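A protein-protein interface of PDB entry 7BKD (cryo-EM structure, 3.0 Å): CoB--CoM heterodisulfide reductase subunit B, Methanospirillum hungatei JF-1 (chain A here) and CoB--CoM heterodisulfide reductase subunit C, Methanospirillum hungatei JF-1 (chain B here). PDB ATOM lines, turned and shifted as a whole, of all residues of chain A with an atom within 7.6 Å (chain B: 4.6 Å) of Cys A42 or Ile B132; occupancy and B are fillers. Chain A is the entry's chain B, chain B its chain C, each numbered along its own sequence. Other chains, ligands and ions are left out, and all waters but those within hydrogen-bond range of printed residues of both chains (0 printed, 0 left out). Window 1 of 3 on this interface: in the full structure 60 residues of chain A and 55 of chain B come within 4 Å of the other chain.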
ATOM      1  N   PHE A   7      -6.119   1.990  -9.587  1.00  0.00           N
ATOM      2  CA  PHE A   7      -7.019   3.141  -9.649  1.00  0.00           C
ATOM      3  C   PHE A   7      -6.279   4.465  -9.509  1.00  0.00           C
ATOM      4  O   PHE A   7      -6.563   5.411 -10.255  1.00  0.00           O
ATOM      5  CB  PHE A   7      -8.106   3.048  -8.586  1.00  0.00           C
ATOM      6  CG  PHE A   7      -8.885   4.317  -8.435  1.00  0.00           C
ATOM      7  CD1 PHE A   7      -9.733   4.738  -9.437  1.00  0.00           C
ATOM      8  CD2 PHE A   7      -8.734   5.114  -7.315  1.00  0.00           C
ATOM      9  CE1 PHE A   7     -10.434   5.910  -9.318  1.00  0.00           C
ATOM     10  CE2 PHE A   7      -9.433   6.290  -7.191  1.00  0.00           C
ATOM     11  CZ  PHE A   7     -10.284   6.687  -8.193  1.00  0.00           C
ATOM     12  N   LEU A   8      -5.349   4.568  -8.555  1.00  0.00           N
ATOM     13  CA  LEU A   8      -4.452   5.721  -8.521  1.00  0.00           C
ATOM     14  C   LEU A   8      -5.168   7.059  -8.378  1.00  0.00           C
ATOM     15  O   LEU A   8      -5.290   7.796  -9.361  1.00  0.00           O
ATOM     16  CB  LEU A   8      -3.579   5.752  -9.774  1.00  0.00           C
ATOM     17  CG  LEU A   8      -2.375   4.838  -9.654  1.00  0.00           C
ATOM     18  CD1 LEU A   8      -1.493   4.981 -10.865  1.00  0.00           C
ATOM     19  CD2 LEU A   8      -1.639   5.192  -8.385  1.00  0.00           C
ATOM     20  N   GLY A   9      -5.657   7.378  -7.184  1.00  0.00           N
ATOM     21  CA  GLY A   9      -6.480   8.560  -7.004  1.00  0.00           C
ATOM     22  C   GLY A   9      -5.706   9.860  -7.105  1.00  0.00           C
ATOM     23  O   GLY A   9      -4.903  10.024  -8.023  1.00  0.00           O
ATOM     24  N   CYS A  10      -5.962  10.822  -6.227  1.00  0.00           N
ATOM     25  CA  CYS A  10      -5.398  12.154  -6.404  1.00  0.00           C
ATOM     26  C   CYS A  10      -4.053  12.349  -5.720  1.00  0.00           C
ATOM     27  O   CYS A  10      -3.079  12.727  -6.379  1.00  0.00           O
ATOM     28  CB  CYS A  10      -6.384  13.216  -5.905  1.00  0.00           C
ATOM     29  SG  CYS A  10      -7.969  13.233  -6.759  1.00  0.00           S
ATOM     30  N   GLY A  39      -8.291   6.573 -17.799  1.00  0.00           N
ATOM     31  CA  GLY A  39      -8.904   7.880 -17.487  1.00  0.00           C
ATOM     32  C   GLY A  39      -9.695   7.890 -16.180  1.00  0.00           C
ATOM     33  O   GLY A  39     -10.816   8.437 -16.168  1.00  0.00           O
ATOM     34  N   ALA A  40      -9.150   7.289 -15.121  1.00  0.00           N
ATOM     35  CA  ALA A  40      -9.800   7.343 -13.794  1.00  0.00           C
ATOM     36  C   ALA A  40      -9.757   8.772 -13.262  1.00  0.00           C
ATOM     37  O   ALA A  40      -8.837   9.494 -13.555  1.00  0.00           O
ATOM     38  CB  ALA A  40      -9.099   6.435 -12.839  1.00  0.00           C
ATOM     39  N   SER A  41     -10.742   9.136 -12.476  1.00  0.00           N
ATOM     40  CA  SER A  41     -10.792  10.496 -11.904  1.00  0.00           C
ATOM     41  C   SER A  41     -10.700  10.396 -10.399  1.00  0.00           C
ATOM     42  O   SER A  41     -10.486   9.290  -9.895  1.00  0.00           O
ATOM     43  CB  SER A  41     -12.117  11.094 -12.208  1.00  0.00           C
ATOM     44  OG  SER A  41     -13.150  10.425 -11.507  1.00  0.00           O
ATOM     45  N   CYS A  42     -10.683  11.534  -9.746  1.00  0.00           N
ATOM     46  CA  CYS A  42     -10.918  11.545  -8.313  1.00  0.00           C
ATOM     47  C   CYS A  42     -12.052  10.592  -7.979  1.00  0.00           C
ATOM     48  O   CYS A  42     -13.179  10.769  -8.450  1.00  0.00           O
ATOM     49  CB  CYS A  42     -11.265  12.962  -7.857  1.00  0.00           C
ATOM     50  SG  CYS A  42     -11.558  13.203  -6.100  1.00  0.00           S
ATOM     51  N   CYS A  43     -11.759   9.567  -7.198  1.00  0.00           N
ATOM     52  CA  CYS A  43     -12.845   8.890  -6.528  1.00  0.00           C
ATOM     53  C   CYS A  43     -13.525   9.963  -5.699  1.00  0.00           C
ATOM     54  O   CYS A  43     -12.835  10.734  -5.022  1.00  0.00           O
ATOM     55  CB  CYS A  43     -12.368   7.743  -5.640  1.00  0.00           C
ATOM     56  SG  CYS A  43     -11.798   8.207  -3.986  1.00  0.00           S
ATOM     57  N   PRO A  44     -14.819  10.118  -5.794  1.00  0.00           N
ATOM     58  CA  PRO A  44     -15.440  11.207  -5.045  1.00  0.00           C
ATOM     59  C   PRO A  44     -15.058  11.041  -3.586  1.00  0.00           C
ATOM     60  O   PRO A  44     -15.511  10.107  -2.916  1.00  0.00           O
ATOM     61  CB  PRO A  44     -16.936  11.016  -5.307  1.00  0.00           C
ATOM     62  CG  PRO A  44     -17.069   9.596  -5.725  1.00  0.00           C
ATOM     63  CD  PRO A  44     -15.804   9.211  -6.399  1.00  0.00           C
ATOM     64  N   ALA A  45     -14.187  11.927  -3.110  1.00  0.00           N
ATOM     65  CA  ALA A  45     -13.588  11.755  -1.798  1.00  0.00           C
ATOM     66  C   ALA A  45     -14.690  11.696  -0.750  1.00  0.00           C
ATOM     67  O   ALA A  45     -15.539  12.593  -0.701  1.00  0.00           O
ATOM     68  CB  ALA A  45     -12.618  12.890  -1.488  1.00  0.00           C
ATOM     69  N   PRO A  46     -14.727  10.657   0.082  1.00  0.00           N
ATOM     70  CA  PRO A  46     -15.913  10.446   0.925  1.00  0.00           C
ATOM     71  C   PRO A  46     -16.193  11.598   1.870  1.00  0.00           C
ATOM     72  O   PRO A  46     -17.363  11.903   2.129  1.00  0.00           O
ATOM     73  CB  PRO A  46     -15.589   9.152   1.680  1.00  0.00           C
ATOM     74  CG  PRO A  46     -14.130   8.943   1.542  1.00  0.00           C
ATOM     75  CD  PRO A  46     -13.604   9.769   0.423  1.00  0.00           C
ATOM     76  N   ALA A  48     -14.706  15.079   1.663  1.00  0.00           N
ATOM     77  CA  ALA A  48     -14.802  16.362   0.983  1.00  0.00           C
ATOM     78  C   ALA A  48     -15.880  16.396  -0.090  1.00  0.00           C
ATOM     79  O   ALA A  48     -16.200  17.484  -0.580  1.00  0.00           O
ATOM     80  CB  ALA A  48     -13.450  16.724   0.366  1.00  0.00           C
ATOM     81  N   PHE A  49     -16.447  15.252  -0.465  1.00  0.00           N
ATOM     82  CA  PHE A  49     -17.422  15.239  -1.546  1.00  0.00           C
ATOM     83  C   PHE A  49     -18.707  14.533  -1.134  1.00  0.00           C
ATOM     84  O   PHE A  49     -19.798  14.918  -1.567  1.00  0.00           O
ATOM     85  CB  PHE A  49     -16.821  14.582  -2.788  1.00  0.00           C
ATOM     86  CG  PHE A  49     -17.335  15.147  -4.070  1.00  0.00           C
ATOM     87  CD1 PHE A  49     -16.917  16.391  -4.501  1.00  0.00           C
ATOM     88  CD2 PHE A  49     -18.238  14.444  -4.843  1.00  0.00           C
ATOM     89  CE1 PHE A  49     -17.387  16.922  -5.681  1.00  0.00           C
ATOM     90  CE2 PHE A  49     -18.707  14.971  -6.024  1.00  0.00           C
ATOM     91  CZ  PHE A  49     -18.283  16.211  -6.443  1.00  0.00           C
ATOM     92  N   VAL A  56     -24.149  12.299  -6.178  1.00  0.00           N
ATOM     93  CA  VAL A  56     -22.989  12.542  -7.030  1.00  0.00           C
ATOM     94  C   VAL A  56     -21.831  11.645  -6.611  1.00  0.00           C
ATOM     95  O   VAL A  56     -21.057  11.173  -7.453  1.00  0.00           O
ATOM     96  CB  VAL A  56     -22.606  14.035  -7.008  1.00  0.00           C
ATOM     97  CG1 VAL A  56     -22.148  14.461  -5.631  1.00  0.00           C
ATOM     98  CG2 VAL A  56     -21.535  14.325  -8.044  1.00  0.00           C
ATOM     99  N   MET A  60     -20.132   9.168  -9.368  1.00  0.00           N
ATOM    100  CA  MET A  60     -18.722   9.230  -9.742  1.00  0.00           C
ATOM    101  C   MET A  60     -17.992   7.944  -9.377  1.00  0.00           C
ATOM    102  O   MET A  60     -17.192   7.430 -10.173  1.00  0.00           O
ATOM    103  CB  MET A  60     -18.052  10.439  -9.096  1.00  0.00           C
ATOM    104  CG  MET A  60     -18.590  11.765  -9.593  1.00  0.00           C
ATOM    105  SD  MET A  60     -17.665  13.172  -8.962  1.00  0.00           S
ATOM    106  CE  MET A  60     -16.023  12.772  -9.546  1.00  0.00           C
ATOM    107  N   ALA A  61     -18.255   7.397  -8.187  1.00  0.00           N
ATOM    108  CA  ALA A  61     -17.617   6.137  -7.831  1.00  0.00           C
ATOM    109  C   ALA A  61     -18.054   5.021  -8.773  1.00  0.00           C
ATOM    110  O   ALA A  61     -17.250   4.160  -9.149  1.00  0.00           O
ATOM    111  CB  ALA A  61     -17.928   5.783  -6.381  1.00  0.00           C
ATOM    112  N   ARG A  63     -18.925   5.414 -11.931  1.00  0.00           N
ATOM    113  CA  ARG A  63     -18.225   5.600 -13.197  1.00  0.00           C
ATOM    114  C   ARG A  63     -16.813   5.039 -13.113  1.00  0.00           C
ATOM    115  O   ARG A  63     -16.332   4.383 -14.048  1.00  0.00           O
ATOM    116  CB  ARG A  63     -18.162   7.076 -13.573  1.00  0.00           C
ATOM    117  CG  ARG A  63     -17.786   7.284 -15.021  1.00  0.00           C
ATOM    118  CD  ARG A  63     -17.560   8.732 -15.335  1.00  0.00           C
ATOM    119  NE  ARG A  63     -16.484   9.240 -14.497  1.00  0.00           N
ATOM    120  CZ  ARG A  63     -15.207   9.241 -14.862  1.00  0.00           C
ATOM    121  NH1 ARG A  63     -14.861   8.769 -16.050  1.00  0.00           N
ATOM    122  NH2 ARG A  63     -14.277   9.710 -14.047  1.00  0.00           N
ATOM    123  N   ASN A  64     -16.131   5.296 -11.995  1.00  0.00           N
ATOM    124  CA  ASN A  64     -14.799   4.735 -11.801  1.00  0.00           C
ATOM    125  C   ASN A  64     -14.839   3.212 -11.818  1.00  0.00           C
ATOM    126  O   ASN A  64     -13.942   2.564 -12.369  1.00  0.00           O
ATOM    127  CB  ASN A  64     -14.200   5.241 -10.490  1.00  0.00           C
ATOM    128  CG  ASN A  64     -13.571   6.610 -10.624  1.00  0.00           C
ATOM    129  OD1 ASN A  64     -12.958   6.930 -11.641  1.00  0.00           O
ATOM    130  ND2 ASN A  64     -13.725   7.429  -9.596  1.00  0.00           N
ATOM    131  N   CYS A  82      -9.893   6.188  -0.833  1.00  0.00           N
ATOM    132  CA  CYS A  82     -10.303   5.663  -2.126  1.00  0.00           C
ATOM    133  C   CYS A  82     -10.949   4.298  -1.969  1.00  0.00           C
ATOM    134  O   CYS A  82     -11.915   3.977  -2.669  1.00  0.00           O
ATOM    135  CB  CYS A  82      -9.103   5.594  -3.070  1.00  0.00           C
ATOM    136  SG  CYS A  82      -8.530   7.192  -3.647  1.00  0.00           S
ATOM    137  N   SER A  85     -14.576   4.959  -0.796  1.00  0.00           N
ATOM    138  CA  SER A  85     -15.437   5.366  -1.902  1.00  0.00           C
ATOM    139  C   SER A  85     -15.724   4.197  -2.844  1.00  0.00           C
ATOM    140  O   SER A  85     -16.874   3.759  -2.982  1.00  0.00           O
ATOM    141  CB  SER A  85     -14.799   6.532  -2.654  1.00  0.00           C
ATOM    142  OG  SER A  85     -15.642   6.981  -3.698  1.00  0.00           O
ATOM    143  N   ILE A  86     -14.678   3.657  -3.474  1.00  0.00           N
ATOM    144  CA  ILE A  86     -14.860   2.687  -4.551  1.00  0.00           C
ATOM    145  C   ILE A  86     -15.504   1.408  -4.026  1.00  0.00           C
ATOM    146  O   ILE A  86     -16.532   0.953  -4.543  1.00  0.00           O
ATOM    147  CB  ILE A  86     -13.509   2.398  -5.233  1.00  0.00           C
ATOM    148  CG1 ILE A  86     -12.905   3.678  -5.812  1.00  0.00           C
ATOM    149  CG2 ILE A  86     -13.662   1.356  -6.316  1.00  0.00           C
ATOM    150  CD1 ILE A  86     -13.813   4.404  -6.760  1.00  0.00           C
ATOM    151  N   PHE A 237      -4.166  10.337   2.333  1.00  0.00           N
ATOM    152  CA  PHE A 237      -4.699  11.339   3.258  1.00  0.00           C
ATOM    153  C   PHE A 237      -3.918  11.376   4.561  1.00  0.00           C
ATOM    154  O   PHE A 237      -3.526  12.453   5.022  1.00  0.00           O
ATOM    155  CB  PHE A 237      -6.176  11.096   3.583  1.00  0.00           C
ATOM    156  CG  PHE A 237      -7.120  11.340   2.453  1.00  0.00           C
ATOM    157  CD1 PHE A 237      -6.728  12.033   1.333  1.00  0.00           C
ATOM    158  CD2 PHE A 237      -8.432  10.911   2.542  1.00  0.00           C
ATOM    159  CE1 PHE A 237      -7.614  12.282   0.311  1.00  0.00           C
ATOM    160  CE2 PHE A 237      -9.325  11.146   1.521  1.00  0.00           C
ATOM    161  CZ  PHE A 237      -8.912  11.835   0.403  1.00  0.00           C
ATOM    162  N   THR B 128     -13.379  22.272  -3.584  1.00  0.00           N
ATOM    163  CA  THR B 128     -13.139  20.926  -4.093  1.00  0.00           C
ATOM    164  C   THR B 128     -14.076  20.606  -5.250  1.00  0.00           C
ATOM    165  O   THR B 128     -13.683  19.941  -6.216  1.00  0.00           O
ATOM    166  CB  THR B 128     -13.303  19.908  -2.963  1.00  0.00           C
ATOM    167  OG1 THR B 128     -12.268  20.106  -1.993  1.00  0.00           O
ATOM    168  CG2 THR B 128     -13.216  18.487  -3.491  1.00  0.00           C
ATOM    169  N   VAL B 129     -15.322  21.076  -5.167  1.00  0.00           N
ATOM    170  CA  VAL B 129     -16.259  20.909  -6.276  1.00  0.00           C
ATOM    171  C   VAL B 129     -15.735  21.611  -7.520  1.00  0.00           C
ATOM    172  O   VAL B 129     -15.779  21.066  -8.627  1.00  0.00           O
ATOM    173  CB  VAL B 129     -17.653  21.426  -5.883  1.00  0.00           C
ATOM    174  CG1 VAL B 129     -18.508  21.654  -7.117  1.00  0.00           C
ATOM    175  CG2 VAL B 129     -18.319  20.445  -4.965  1.00  0.00           C
ATOM    176  N   GLN B 130     -15.240  22.839  -7.352  1.00  0.00           N
ATOM    177  CA  GLN B 130     -14.656  23.570  -8.473  1.00  0.00           C
ATOM    178  C   GLN B 130     -13.518  22.777  -9.104  1.00  0.00           C
ATOM    179  O   GLN B 130     -13.453  22.622 -10.330  1.00  0.00           O
ATOM    180  CB  GLN B 130     -14.147  24.933  -8.000  1.00  0.00           C
ATOM    181  CG  GLN B 130     -15.211  25.863  -7.448  1.00  0.00           C
ATOM    182  CD  GLN B 130     -16.172  26.353  -8.506  1.00  0.00           C
ATOM    183  OE1 GLN B 130     -17.340  25.973  -8.521  1.00  0.00           O
ATOM    184  NE2 GLN B 130     -15.686  27.208  -9.396  1.00  0.00           N
ATOM    185  N   LEU B 131     -12.615  22.261  -8.269  1.00  0.00           N
ATOM    186  CA  LEU B 131     -11.455  21.532  -8.772  1.00  0.00           C
ATOM    187  C   LEU B 131     -11.871  20.274  -9.524  1.00  0.00           C
ATOM    188  O   LEU B 131     -11.358  19.988 -10.612  1.00  0.00           O
ATOM    189  CB  LEU B 131     -10.525  21.175  -7.613  1.00  0.00           C
ATOM    190  CG  LEU B 131      -9.762  22.324  -6.965  1.00  0.00           C
ATOM    191  CD1 LEU B 131      -9.299  21.923  -5.577  1.00  0.00           C
ATOM    192  CD2 LEU B 131      -8.585  22.737  -7.828  1.00  0.00           C
ATOM    193  N   ILE B 132     -12.800  19.504  -8.955  1.00  0.00           N
ATOM    194  CA  ILE B 132     -13.215  18.256  -9.588  1.00  0.00           C
ATOM    195  C   ILE B 132     -13.965  18.538 -10.881  1.00  0.00           C
ATOM    196  O   ILE B 132     -13.821  17.812 -11.870  1.00  0.00           O
ATOM    197  CB  ILE B 132     -14.051  17.412  -8.608  1.00  0.00           C
ATOM    198  CG1 ILE B 132     -13.148  16.771  -7.558  1.00  0.00           C
ATOM    199  CG2 ILE B 132     -14.831  16.335  -9.345  1.00  0.00           C
ATOM    200  CD1 ILE B 132     -13.896  16.131  -6.413  1.00  0.00           C
ATOM    201  N   TYR B 133     -14.771  19.598 -10.905  1.00  0.00           N
ATOM    202  CA  TYR B 133     -15.474  19.952 -12.131  1.00  0.00           C
ATOM    203  C   TYR B 133     -14.497  20.365 -13.222  1.00  0.00           C
ATOM    204  O   TYR B 133     -14.682  20.013 -14.393  1.00  0.00           O
ATOM    205  CB  TYR B 133     -16.472  21.070 -11.853  1.00  0.00           C
ATOM    206  CG  TYR B 133     -17.388  21.366 -13.010  1.00  0.00           C
ATOM    207  CD1 TYR B 133     -18.561  20.649 -13.187  1.00  0.00           C
ATOM    208  CD2 TYR B 133     -17.078  22.353 -13.930  1.00  0.00           C
ATOM    209  CE1 TYR B 133     -19.400  20.914 -14.241  1.00  0.00           C
ATOM    210  CE2 TYR B 133     -17.912  22.621 -14.990  1.00  0.00           C
ATOM    211  CZ  TYR B 133     -19.071  21.900 -15.140  1.00  0.00           C
ATOM    212  OH  TYR B 133     -19.908  22.166 -16.197  1.00  0.00           O
ATOM    213  N   ASN B 134     -13.455  21.115 -12.862  1.00  0.00           N
ATOM    214  CA  ASN B 134     -12.518  21.598 -13.872  1.00  0.00           C
ATOM    215  C   ASN B 134     -11.623  20.476 -14.389  1.00  0.00           C
ATOM    216  O   ASN B 134     -11.391  20.363 -15.598  1.00  0.00           O
ATOM    217  CB  ASN B 134     -11.678  22.737 -13.298  1.00  0.00           C
ATOM    218  CG  ASN B 134     -12.506  23.966 -12.977  1.00  0.00           C
ATOM    219  OD1 ASN B 134     -13.529  24.224 -13.610  1.00  0.00           O
ATOM    220  ND2 ASN B 134     -12.063  24.738 -11.991  1.00  0.00           N
ATOM    221  N   SER B 135     -11.105  19.639 -13.490  1.00  0.00           N
ATOM    222  CA  SER B 135     -10.083  18.667 -13.849  1.00  0.00           C
ATOM    223  C   SER B 135     -10.414  17.228 -13.486  1.00  0.00           C
ATOM    224  O   SER B 135      -9.644  16.332 -13.849  1.00  0.00           O
ATOM    225  CB  SER B 135      -8.747  19.038 -13.190  1.00  0.00           C
ATOM    226  OG  SER B 135      -8.758  18.720 -11.811  1.00  0.00           O
ATOM    227  N   GLY B 136     -11.513  16.971 -12.782  1.00  0.00           N
ATOM    228  CA  GLY B 136     -11.777  15.626 -12.313  1.00  0.00           C
ATOM    229  C   GLY B 136     -10.955  15.194 -11.121  1.00  0.00           C
ATOM    230  O   GLY B 136     -10.958  14.010 -10.780  1.00  0.00           O
ATOM    231  N   HIS B 137     -10.212  16.106 -10.481  1.00  0.00           N
ATOM    232  CA  HIS B 137      -9.314  15.754  -9.339  1.00  0.00           C
ATOM    233  C   HIS B 137      -9.436  16.748  -8.171  1.00  0.00           C
ATOM    234  O   HIS B 137      -9.028  17.900  -8.375  1.00  0.00           O
ATOM    235  CB  HIS B 137      -7.849  15.640  -9.780  1.00  0.00           C
ATOM    236  CG  HIS B 137      -7.402  14.319 -10.299  1.00  0.00           C
ATOM    237  ND1 HIS B 137      -8.080  13.147 -10.053  1.00  0.00           N
ATOM    238  CD2 HIS B 137      -6.323  13.982 -11.032  1.00  0.00           C
ATOM    239  CE1 HIS B 137      -7.442  12.147 -10.618  1.00  0.00           C
ATOM    240  NE2 HIS B 137      -6.357  12.632 -11.216  1.00  0.00           N
ATOM    241  N   GLY B 138      -9.950  16.346  -6.988  1.00  0.00           N
ATOM    242  CA  GLY B 138      -9.988  17.220  -5.834  1.00  0.00           C
ATOM    243  C   GLY B 138      -8.618  17.684  -5.398  1.00  0.00           C
ATOM    244  O   GLY B 138      -8.492  18.735  -4.765  1.00  0.00           O
ATOM    245  N   ILE B 171     -17.656  13.610 -16.584  1.00  0.00           N
ATOM    246  CA  ILE B 171     -17.756  13.891 -15.157  1.00  0.00           C
ATOM    247  C   ILE B 171     -18.595  15.135 -14.939  1.00  0.00           C
ATOM    248  O   ILE B 171     -19.506  15.150 -14.102  1.00  0.00           O
ATOM    249  CB  ILE B 171     -16.358  14.046 -14.534  1.00  0.00           C
ATOM    250  CG1 ILE B 171     -15.541  12.770 -14.707  1.00  0.00           C
ATOM    251  CG2 ILE B 171     -16.471  14.398 -13.060  1.00  0.00           C
ATOM    252  CD1 ILE B 171     -14.069  12.977 -14.472  1.00  0.00           C
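Ser A41 touches Gly B136 (CB to O, 3.4 Å). Ser A41 touches His B137. Ile B171 touches Ser A41. Cys A42 touches Ile B132 (SG to CD1, 3.8 Å). Phe A49 touches Val B129. CD1 of Ile B132 touches CD1 of Phe A49, 3.6 Å away. Met A60 touches Ile B132. CE of Met A60 touches CG2 of Ile B171, at 3.9 Å. NH2 of Arg A63 touches CD1 of Ile B171, 3.3 Å away.
Of the 12 printed residues of chain B, 6 touch a printed residue of chain A. Printed residues of chain B that touch a printed residue of chain A: Val B129, Ile B132, Gly B136, His B137, Gly B138 and Ile B171. Hydrophobic or aromatic side chains of chain B that line the printed part of chain A: Val B129, Ile B132, His B137 and Ile B171. Printed residues of chain A that touch a printed residue of chain B: Cys A10, Ser A41, Cys A42, Phe A49, Met A60 and Arg A63. Among the printed residues, no Asp or Glu carboxylate lies within 4 Å of a Lys or Arg side-chain nitrogen of the other chain.
The backbone carbonyl oxygen (O) of Gly B136 is in hydrogen-bond range of the backbone NH (N) of Cys A42, at 2.7 Å. SG of Cys A10 sits close to ND1 of His B137 (3.3 Å). The backbone NH (N) of Cys A42 is in hydrogen-bond range of a ring nitrogen (ND1) of His B137 (3.1 Å). The side-chain sulfur of Cys A10 lies close to the backbone NH of Gly B138, 3.7 Å away. The backbone NH of Gly B138 lies close to the side-chain sulfur of Cys A42, 3.6 Å away.
Of chain B, only Ile B132, Gly B136, His B137 and Gly B138 come within 4 Å of Cys A42. Ile B132 touches just these residues of chain A: Cys A42, Phe A49 and Met A60. Of the printed residues of chain A, His B137 touches Cys A10, Ser A41 and Cys A42. Printed residues of chain A within 4 Å of Gly B136: Ser A41 (3.4 Å) and Cys A42 (2.7 Å). Printed residues of chain B within 4 Å of Phe A49: Val B129 and Ile B132. Of the printed residues of chain B, Cys A10 touches His B137 (3.3 Å) and Gly B138 (3.7 Å). The nearest printed residue of chain B that does not touch Cys A42 is Ile B171 (6.0 Å). The nearest printed residue of chain A that does not touch Ile B132 is Pro A44 (5.3 Å).
The side-chain hydroxyl of Ser B135 lies close to the backbone NH of His B137, 3.3 Å away. The side-chain hydroxyl of Ser A41 lies within hydrogen-bond range of the guanidinium group of Arg A63 (2.9 Å). OD1 of Asn A64 sits at hydrogen-bond distance from N of Ser A41 (3.2 Å).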
